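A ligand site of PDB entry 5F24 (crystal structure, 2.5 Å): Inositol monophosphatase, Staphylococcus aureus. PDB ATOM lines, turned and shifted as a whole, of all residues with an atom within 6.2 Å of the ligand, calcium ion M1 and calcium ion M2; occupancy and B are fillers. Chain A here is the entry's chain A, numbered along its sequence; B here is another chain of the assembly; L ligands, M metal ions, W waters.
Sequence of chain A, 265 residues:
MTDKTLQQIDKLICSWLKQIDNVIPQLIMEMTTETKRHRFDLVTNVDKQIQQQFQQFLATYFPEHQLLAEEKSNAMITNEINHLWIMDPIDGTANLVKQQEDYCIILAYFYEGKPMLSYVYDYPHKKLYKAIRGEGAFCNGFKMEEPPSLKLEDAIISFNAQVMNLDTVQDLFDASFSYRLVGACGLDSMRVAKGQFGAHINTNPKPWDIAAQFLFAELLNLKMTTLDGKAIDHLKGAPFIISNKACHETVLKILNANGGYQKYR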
ATOM      1  N   ASP A  47      15.819  10.512   2.958  1.00  0.00           N
ATOM      2  CA  ASP A  47      14.570  10.901   3.618  1.00  0.00           C
ATOM      3  C   ASP A  47      13.795   9.663   4.043  1.00  0.00           C
ATOM      4  O   ASP A  47      13.383   9.561   5.199  1.00  0.00           O
ATOM      5  CB  ASP A  47      13.700  11.764   2.696  1.00  0.00           C
ATOM      6  CG  ASP A  47      14.424  12.996   2.158  1.00  0.00           C
ATOM      7  OD1 ASP A  47      15.505  12.853   1.524  1.00  0.00           O
ATOM      8  OD2 ASP A  47      13.883  14.116   2.289  1.00  0.00           O
ATOM      9  N   GLU A  70       6.538  13.964   6.611  1.00  0.00           N
ATOM     10  CA  GLU A  70       6.467  14.372   5.192  1.00  0.00           C
ATOM     11  C   GLU A  70       6.201  13.199   4.280  1.00  0.00           C
ATOM     12  O   GLU A  70       5.357  13.250   3.393  1.00  0.00           O
ATOM     13  CB  GLU A  70       7.742  15.102   4.744  1.00  0.00           C
ATOM     14  CG  GLU A  70       7.669  15.560   3.267  1.00  0.00           C
ATOM     15  CD  GLU A  70       8.693  16.632   2.940  1.00  0.00           C
ATOM     16  OE1 GLU A  70       8.616  17.175   1.833  1.00  0.00           O
ATOM     17  OE2 GLU A  70       9.549  16.911   3.808  1.00  0.00           O
ATOM     18  N   GLU A  71       6.956  12.119   4.461  1.00  0.00           N
ATOM     19  CA  GLU A  71       6.996  11.019   3.471  1.00  0.00           C
ATOM     20  C   GLU A  71       5.908   9.939   3.713  1.00  0.00           C
ATOM     21  O   GLU A  71       6.028   8.819   3.296  1.00  0.00           O
ATOM     22  CB  GLU A  71       8.390  10.334   3.429  1.00  0.00           C
ATOM     23  CG  GLU A  71       9.605  11.273   3.348  1.00  0.00           C
ATOM     24  CD  GLU A  71       9.554  12.271   2.189  1.00  0.00           C
ATOM     25  OE1 GLU A  71       8.998  11.929   1.110  1.00  0.00           O
ATOM     26  OE2 GLU A  71      10.062  13.388   2.378  1.00  0.00           O
ATOM     27  N   ASP A  88      10.272  16.030  10.047  1.00  0.00           N
ATOM     28  CA  ASP A  88      10.829  16.189   8.708  1.00  0.00           C
ATOM     29  C   ASP A  88      12.139  15.409   8.649  1.00  0.00           C
ATOM     30  O   ASP A  88      13.156  15.768   9.294  1.00  0.00           O
ATOM     31  CB  ASP A  88      11.050  17.620   8.286  1.00  0.00           C
ATOM     32  CG  ASP A  88      11.261  17.755   6.798  1.00  0.00           C
ATOM     33  OD1 ASP A  88      11.688  16.754   6.180  1.00  0.00           O
ATOM     34  OD2 ASP A  88      11.002  18.866   6.254  1.00  0.00           O
ATOM     35  N   PRO A  89      12.126  14.279   7.963  1.00  0.00           N
ATOM     36  CA  PRO A  89      13.304  13.387   8.100  1.00  0.00           C
ATOM     37  C   PRO A  89      14.552  13.990   7.486  1.00  0.00           C
ATOM     38  O   PRO A  89      15.637  13.764   8.018  1.00  0.00           O
ATOM     39  CB  PRO A  89      12.871  12.110   7.379  1.00  0.00           C
ATOM     40  CG  PRO A  89      11.766  12.534   6.467  1.00  0.00           C
ATOM     41  CD  PRO A  89      11.070  13.651   7.161  1.00  0.00           C
ATOM     42  N   ILE A  90      14.427  14.697   6.381  1.00  0.00           N
ATOM     43  CA  ILE A  90      15.478  15.617   5.925  1.00  0.00           C
ATOM     44  C   ILE A  90      14.819  16.949   5.561  1.00  0.00           C
ATOM     45  O   ILE A  90      14.019  17.015   4.646  1.00  0.00           O
ATOM     46  CB  ILE A  90      16.203  15.080   4.690  1.00  0.00           C
ATOM     47  CG1 ILE A  90      16.952  13.804   5.037  1.00  0.00           C
ATOM     48  CG2 ILE A  90      17.167  16.130   4.162  1.00  0.00           C
ATOM     49  CD1 ILE A  90      18.141  13.998   5.968  1.00  0.00           C
ATOM     50  N   ASP A  91      15.163  17.986   6.294  1.00  0.00           N
ATOM     51  CA  ASP A  91      14.745  19.346   5.905  1.00  0.00           C
ATOM     52  C   ASP A  91      15.925  19.922   5.203  1.00  0.00           C
ATOM     53  O   ASP A  91      16.990  19.895   5.736  1.00  0.00           O
ATOM     54  CB  ASP A  91      14.322  20.187   7.100  1.00  0.00           C
ATOM     55  CG  ASP A  91      13.863  21.593   6.726  1.00  0.00           C
ATOM     56  OD1 ASP A  91      13.008  21.741   5.825  1.00  0.00           O
ATOM     57  OD2 ASP A  91      14.407  22.547   7.320  1.00  0.00           O
ATOM     58  N   GLY A  92      15.742  20.465   4.028  1.00  0.00           N
ATOM     59  CA  GLY A  92      16.868  20.889   3.164  1.00  0.00           C
ATOM     60  C   GLY A  92      17.351  19.843   2.180  1.00  0.00           C
ATOM     61  O   GLY A  92      18.565  19.659   1.965  1.00  0.00           O
ATOM     62  N   THR A  93      16.416  19.097   1.614  1.00  0.00           N
ATOM     63  CA  THR A  93      16.731  17.985   0.685  1.00  0.00           C
ATOM     64  C   THR A  93      17.543  18.524  -0.496  1.00  0.00           C
ATOM     65  O   THR A  93      18.463  17.868  -0.968  1.00  0.00           O
ATOM     66  CB  THR A  93      15.408  17.281   0.237  1.00  0.00           C
ATOM     67  OG1 THR A  93      14.816  16.591   1.368  1.00  0.00           O
ATOM     68  CG2 THR A  93      15.625  16.266  -0.812  1.00  0.00           C
ATOM     69  N   ALA A  94      17.225  19.722  -0.975  1.00  0.00           N
ATOM     70  CA  ALA A  94      17.959  20.318  -2.081  1.00  0.00           C
ATOM     71  C   ALA A  94      19.419  20.479  -1.700  1.00  0.00           C
ATOM     72  O   ALA A  94      20.301  20.085  -2.462  1.00  0.00           O
ATOM     73  CB  ALA A  94      17.356  21.653  -2.475  1.00  0.00           C
ATOM     74  N   ILE A 106      14.312  17.237  11.590  1.00  0.00           N
ATOM     75  CA  ILE A 106      13.413  17.945  12.497  1.00  0.00           C
ATOM     76  C   ILE A 106      12.414  16.964  13.179  1.00  0.00           C
ATOM     77  O   ILE A 106      11.730  16.202  12.516  1.00  0.00           O
ATOM     78  CB  ILE A 106      12.646  19.034  11.724  1.00  0.00           C
ATOM     79  CG1 ILE A 106      13.599  20.005  11.028  1.00  0.00           C
ATOM     80  CG2 ILE A 106      11.771  19.856  12.660  1.00  0.00           C
ATOM     81  CD1 ILE A 106      12.923  21.118  10.255  1.00  0.00           C
ATOM     82  N   ASN A 160      13.118  33.215   1.271  1.00  0.00           N
ATOM     83  CA  ASN A 160      13.220  32.837  -0.142  1.00  0.00           C
ATOM     84  C   ASN A 160      12.769  34.017  -0.984  1.00  0.00           C
ATOM     85  O   ASN A 160      11.572  34.334  -1.029  1.00  0.00           O
ATOM     86  CB  ASN A 160      12.354  31.624  -0.461  1.00  0.00           C
ATOM     87  CG  ASN A 160      12.489  31.162  -1.909  1.00  0.00           C
ATOM     88  OD1 ASN A 160      13.090  31.838  -2.720  1.00  0.00           O
ATOM     89  ND2 ASN A 160      11.908  30.004  -2.230  1.00  0.00           N
ATOM     90  N   LEU A 181      20.956  33.312   3.197  1.00  0.00           N
ATOM     91  CA  LEU A 181      20.084  32.137   3.141  1.00  0.00           C
ATOM     92  C   LEU A 181      20.906  30.878   3.324  1.00  0.00           C
ATOM     93  O   LEU A 181      21.760  30.548   2.506  1.00  0.00           O
ATOM     94  CB  LEU A 181      19.312  32.096   1.825  1.00  0.00           C
ATOM     95  CG  LEU A 181      18.266  30.978   1.675  1.00  0.00           C
ATOM     96  CD1 LEU A 181      17.206  30.987   2.740  1.00  0.00           C
ATOM     97  CD2 LEU A 181      17.593  31.088   0.319  1.00  0.00           C
ATOM     98  N   GLY A 183      19.069  27.877   3.602  1.00  0.00           N
ATOM     99  CA  GLY A 183      18.271  27.104   2.649  1.00  0.00           C
ATOM    100  C   GLY A 183      17.602  25.873   3.249  1.00  0.00           C
ATOM    101  O   GLY A 183      17.162  24.976   2.531  1.00  0.00           O
ATOM    102  N   ALA A 184      17.623  25.767   4.555  1.00  0.00           N
ATOM    103  CA  ALA A 184      16.800  24.762   5.235  1.00  0.00           C
ATOM    104  C   ALA A 184      16.022  25.442   6.320  1.00  0.00           C
ATOM    105  O   ALA A 184      16.617  26.005   7.222  1.00  0.00           O
ATOM    106  CB  ALA A 184      17.636  23.645   5.802  1.00  0.00           C
ATOM    107  N   CYS A 185      14.692  25.364   6.282  1.00  0.00           N
ATOM    108  CA  CYS A 185      13.836  26.085   7.253  1.00  0.00           C
ATOM    109  C   CYS A 185      14.289  25.895   8.698  1.00  0.00           C
ATOM    110  O   CYS A 185      14.386  26.878   9.439  1.00  0.00           O
ATOM    111  CB  CYS A 185      12.409  25.648   7.118  1.00  0.00           C
ATOM    112  SG  CYS A 185      11.245  26.648   8.082  1.00  0.00           S
ATOM    113  N   GLY A 186      14.531  24.662   9.096  1.00  0.00           N
ATOM    114  CA  GLY A 186      15.050  24.362  10.416  1.00  0.00           C
ATOM    115  C   GLY A 186      16.342  25.085  10.767  1.00  0.00           C
ATOM    116  O   GLY A 186      16.537  25.553  11.905  1.00  0.00           O
ATOM    117  N   ASP A 188      17.815  27.862   9.091  1.00  0.00           N
ATOM    118  CA  ASP A 188      17.581  29.279   9.068  1.00  0.00           C
ATOM    119  C   ASP A 188      16.818  29.718  10.326  1.00  0.00           C
ATOM    120  O   ASP A 188      17.104  30.767  10.899  1.00  0.00           O
ATOM    121  CB  ASP A 188      16.798  29.683   7.829  1.00  0.00           C
ATOM    122  CG  ASP A 188      17.632  29.614   6.549  1.00  0.00           C
ATOM    123  OD1 ASP A 188      18.435  30.522   6.327  1.00  0.00           O
ATOM    124  OD2 ASP A 188      17.441  28.691   5.733  1.00  0.00           O
ATOM    125  N   HIS A 200      13.504  34.788  10.136  1.00  0.00           N
ATOM    126  CA  HIS A 200      13.385  33.926   8.991  1.00  0.00           C
ATOM    127  C   HIS A 200      11.924  33.883   8.576  1.00  0.00           C
ATOM    128  O   HIS A 200      11.045  33.768   9.446  1.00  0.00           O
ATOM    129  CB  HIS A 200      13.962  32.530   9.256  1.00  0.00           C
ATOM    130  CG  HIS A 200      13.739  31.573   8.129  1.00  0.00           C
ATOM    131  ND1 HIS A 200      14.322  31.723   6.895  1.00  0.00           N
ATOM    132  CD2 HIS A 200      12.944  30.470   8.030  1.00  0.00           C
ATOM    133  CE1 HIS A 200      13.927  30.747   6.086  1.00  0.00           C
ATOM    134  NE2 HIS A 200      13.070  29.987   6.752  1.00  0.00           N
ATOM    135  N   ASN A 202       9.054  31.969   5.939  1.00  0.00           N
ATOM    136  CA  ASN A 202       8.675  30.985   4.943  1.00  0.00           C
ATOM    137  C   ASN A 202       7.190  31.175   4.590  1.00  0.00           C
ATOM    138  O   ASN A 202       6.285  31.007   5.439  1.00  0.00           O
ATOM    139  CB  ASN A 202       8.873  29.572   5.447  1.00  0.00           C
ATOM    140  CG  ASN A 202       8.627  28.521   4.358  1.00  0.00           C
ATOM    141  OD1 ASN A 202       7.602  28.540   3.673  1.00  0.00           O
ATOM    142  ND2 ASN A 202       9.558  27.594   4.205  1.00  0.00           N
ATOM    143  N   ASN A 204       5.100  29.542   2.767  1.00  0.00           N
ATOM    144  CA  ASN A 204       4.208  28.407   2.595  1.00  0.00           C
ATOM    145  C   ASN A 204       4.761  27.112   3.225  1.00  0.00           C
ATOM    146  O   ASN A 204       5.045  26.153   2.503  1.00  0.00           O
ATOM    147  CB  ASN A 204       4.008  28.172   1.105  1.00  0.00           C
ATOM    148  CG  ASN A 204       2.878  27.195   0.792  1.00  0.00           C
ATOM    149  OD1 ASN A 204       2.761  26.753  -0.345  1.00  0.00           O
ATOM    150  ND2 ASN A 204       2.037  26.906   1.758  1.00  0.00           N
ATOM    151  N   PRO A 205       4.962  27.113   4.540  1.00  0.00           N
ATOM    152  CA  PRO A 205       5.510  25.900   5.174  1.00  0.00           C
ATOM    153  C   PRO A 205       4.514  24.799   5.446  1.00  0.00           C
ATOM    154  O   PRO A 205       3.366  25.062   5.664  1.00  0.00           O
ATOM    155  CB  PRO A 205       5.990  26.439   6.512  1.00  0.00           C
ATOM    156  CG  PRO A 205       4.987  27.502   6.836  1.00  0.00           C
ATOM    157  CD  PRO A 205       4.661  28.163   5.525  1.00  0.00           C
ATOM    158  N   TRP A 208       5.591  20.068   9.237  1.00  0.00           N
ATOM    159  CA  TRP A 208       6.923  19.499   9.578  1.00  0.00           C
ATOM    160  C   TRP A 208       8.056  20.484   9.435  1.00  0.00           C
ATOM    161  O   TRP A 208       9.063  20.337  10.110  1.00  0.00           O
ATOM    162  CB  TRP A 208       7.213  18.187   8.878  1.00  0.00           C
ATOM    163  CG  TRP A 208       6.801  18.167   7.482  1.00  0.00           C
ATOM    164  CD1 TRP A 208       7.502  18.620   6.421  1.00  0.00           C
ATOM    165  CD2 TRP A 208       5.581  17.646   6.971  1.00  0.00           C
ATOM    166  NE1 TRP A 208       6.793  18.441   5.277  1.00  0.00           N
ATOM    167  CE2 TRP A 208       5.605  17.867   5.579  1.00  0.00           C
ATOM    168  CE3 TRP A 208       4.455  17.054   7.547  1.00  0.00           C
ATOM    169  CZ2 TRP A 208       4.543  17.481   4.746  1.00  0.00           C
ATOM    170  CZ3 TRP A 208       3.386  16.670   6.707  1.00  0.00           C
ATOM    171  CH2 TRP A 208       3.445  16.884   5.321  1.00  0.00           C
ATOM    172  N   ASP A 209       7.935  21.478   8.563  1.00  0.00           N
ATOM    173  CA  ASP A 209       8.964  22.527   8.404  1.00  0.00           C
ATOM    174  C   ASP A 209       9.128  23.413   9.615  1.00  0.00           C
ATOM    175  O   ASP A 209      10.221  23.997   9.846  1.00  0.00           O
ATOM    176  CB  ASP A 209       8.521  23.521   7.321  1.00  0.00           C
ATOM    177  CG  ASP A 209       8.635  22.973   5.927  1.00  0.00           C
ATOM    178  OD1 ASP A 209       9.655  22.338   5.612  1.00  0.00           O
ATOM    179  OD2 ASP A 209       7.677  23.187   5.146  1.00  0.00           O
ATOM    180  N   ARG B 180      21.552  30.531  -3.089  1.00  0.00           N
ATOM    181  CA  ARG B 180      22.002  30.565  -1.700  1.00  0.00           C
ATOM    182  C   ARG B 180      23.037  31.622  -1.543  1.00  0.00           C
ATOM    183  O   ARG B 180      23.624  32.085  -2.505  1.00  0.00           O
ATOM    184  CB  ARG B 180      22.618  29.275  -1.121  1.00  0.00           C
ATOM    185  CG  ARG B 180      21.968  27.926  -1.374  1.00  0.00           C
ATOM    186  CD  ARG B 180      20.990  27.427  -0.318  1.00  0.00           C
ATOM    187  NE  ARG B 180      19.702  27.563  -0.949  1.00  0.00           N
ATOM    188  CZ  ARG B 180      18.844  26.616  -1.274  1.00  0.00           C
ATOM    189  NH1 ARG B 180      18.972  25.344  -0.949  1.00  0.00           N
ATOM    190  NH2 ARG B 180      17.791  27.005  -1.921  1.00  0.00           N
HETATM  191  C1  LIG L   1      12.133  22.758   2.274  1.00  0.00           C
HETATM  192  C2  LIG L   1      13.243  23.556   2.956  1.00  0.00           C
HETATM  193  C3  LIG L   1      13.495  24.843   2.177  1.00  0.00           C
HETATM  194  C4  LIG L   1      12.268  25.589   1.586  1.00  0.00           C
HETATM  195  C5  LIG L   1      10.918  24.876   1.559  1.00  0.00           C
HETATM  196  C6  LIG L   1      10.841  23.538   2.297  1.00  0.00           C
HETATM  197  P1  LIG L   1      12.523  20.097   2.283  1.00  0.00           P
HETATM  198  O1  LIG L   1      11.920  21.494   2.898  1.00  0.00           O
HETATM  199  O2  LIG L   1      13.009  23.777   4.352  1.00  0.00           O
HETATM  200  O3  LIG L   1      14.400  25.749   2.816  1.00  0.00           O
HETATM  201  O4  LIG L   1      12.145  26.941   2.043  1.00  0.00           O
HETATM  202  O5  LIG L   1       9.918  25.752   2.043  1.00  0.00           O
HETATM  203  O6  LIG L   1       9.849  22.803   1.584  1.00  0.00           O
HETATM  204  O7  LIG L   1      13.979  20.402   2.127  1.00  0.00           O
HETATM  205  O8  LIG L   1      12.080  19.174   3.397  1.00  0.00           O
HETATM  206  O9  LIG L   1      11.859  19.915   0.936  1.00  0.00           O
HETATM  207 CA    CA M   1      11.119  20.720   4.895  1.00  0.00          CA
HETATM  208 CA    CA M   2      11.849  16.926   3.863  1.00  0.00          CA
HETATM  209  O   HOH W   1       9.284  19.878   3.709  1.00  0.00           O
HETATM  210  O   HOH W   2      15.024  28.160   4.168  1.00  0.00           O
HETATM  211  O   HOH W   3      12.284  28.139   4.970  1.00  0.00           O
HETATM  212  O   HOH W   4      12.274  17.214   1.603  1.00  0.00           O
HETATM  213  O   HOH W   5      15.199  21.677   0.214  1.00  0.00           O
HETATM  214  O   HOH W   6      12.097  14.685   3.642  1.00  0.00           O
HETATM  215  O   HOH W   7      14.012  28.995   1.810  1.00  0.00           O
HETATM  216  O   HOH W   8       7.869  22.050   2.730  1.00  0.00           O
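Calcium ion M1 is bound by an oxygen (O1) of the ligand (2.3 Å).
OD1 of Asp 209 is bound to calcium ion M1, 2.3 Å away.
Calcium ion M1 is bound by the side-chain carboxylate (OD2) of Asp 88 (2.3 Å).
OD1 of Asp 91 is bound to calcium ion M1, 2.3 Å away.
Calcium ion M1 is bound by water W1 (2.3 Å).
An oxygen (O8) of the ligand binds calcium ion M1 (2.4 Å).
Three residues have an atom within 4 Å of calcium ion M1: Asp 88, Asp 91 and Asp 209.
The nearest printed residue that does not touch calcium ion M1 is Glu 70 (4.3 Å).
Calcium ion M2 is bound by water W6 (2.3 Å), OE2 of Glu 70 (2.3 Å), O8 of the ligand (2.3 Å), O of Ile 90 (2.3 Å), water W4 (2.3 Å) and OD1 of Asp 88 (2.3 Å).
Calcium ion M2 has six donor atoms within binding distance.
Ala 184 touches the ligand.
Of the 25 residues printed, 11 come within 4 Å of the ligand.
The nearest printed residue that does not touch the ligand is Ala 94 (4.5 Å).
Merely in contact with calcium ion M2: Asp 47 and Thr 93.
The nearest printed residue that does not touch calcium ion M2 is Glu 71 (4.2 Å).
The backbone carbonyl oxygen (O) of Asp 209 lies within hydrogen-bond range of the side-chain sulfur (SG) of Cys 185 (3.3 Å).
The indole nitrogen of Trp 208 lies close to the side-chain carboxylate of Glu 70 (3.5 Å).
The backbone NH (N) of Asp 88 lies within hydrogen-bond range of the backbone carbonyl oxygen (O) of Ile 106 (2.9 Å).
O of Ile 90 lies close to OG1 of Thr 93 (3.4 Å).
N of Gly 186 lies within hydrogen-bond range of OD2 of Asp 91, 2.8 Å away.
N of Asn 204 lies within hydrogen-bond range of OD1 of Asn 202 (2.8 Å).
N of Gly 183 lies within hydrogen-bond range of OD2 of Asp 188 (2.8 Å).
The side-chain carboxylate of Asp 188 lies within hydrogen-bond range of the backbone NH of Ala 184, at 3.2 Å.
An oxygen (O7) of the ligand is in hydrogen-bond range of the backbone NH (N) of Gly 92 (2.6 Å).
An oxygen (O7) of the ligand sits at hydrogen-bond distance from the backbone NH (N) of Thr 93 (2.8 Å).
The side-chain amide nitrogen (ND2) of Asn 202 sits at hydrogen-bond distance from an oxygen (O5) of the ligand (2.9 Å).
O of Gly 183 sits at hydrogen-bond distance from O3 of the ligand, 2.9 Å away.
The backbone NH (N) of Cys 185 lies within hydrogen-bond range of an oxygen (O2) of the ligand, 3.0 Å away.
Water W1 bridges NE1 of Trp 208 (3.3 Å) and OE1 of Glu 70 (3.4 Å).
Water W4 lies within hydrogen-bond range of the side-chain hydroxyl of Thr 93 (2.6 Å) and an oxygen (O9) of the ligand (2.8 Å).
Water W8 bridges O6 of the ligand (2.4 Å) and OD2 of Asp 209 (2.7 Å).
Water W5 lies within hydrogen-bond range of an oxygen (O7) of the ligand (2.6 Å), the backbone NH (N) of Ala 94 (3.1 Å) and the backbone NH (N) of Thr 93 (3.2 Å).
Water W2 bridges an oxygen (O3) of the ligand (2.8 Å) and the side-chain carboxylate of Asp 188 (2.9 Å).
Water W3 lies within hydrogen-bond range of NE2 of His 200 (2.7 Å), ND2 of Asn 202 (2.9 Å), O4 of the ligand (3.2 Å) and SG of Cys 185 (3.6 Å).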
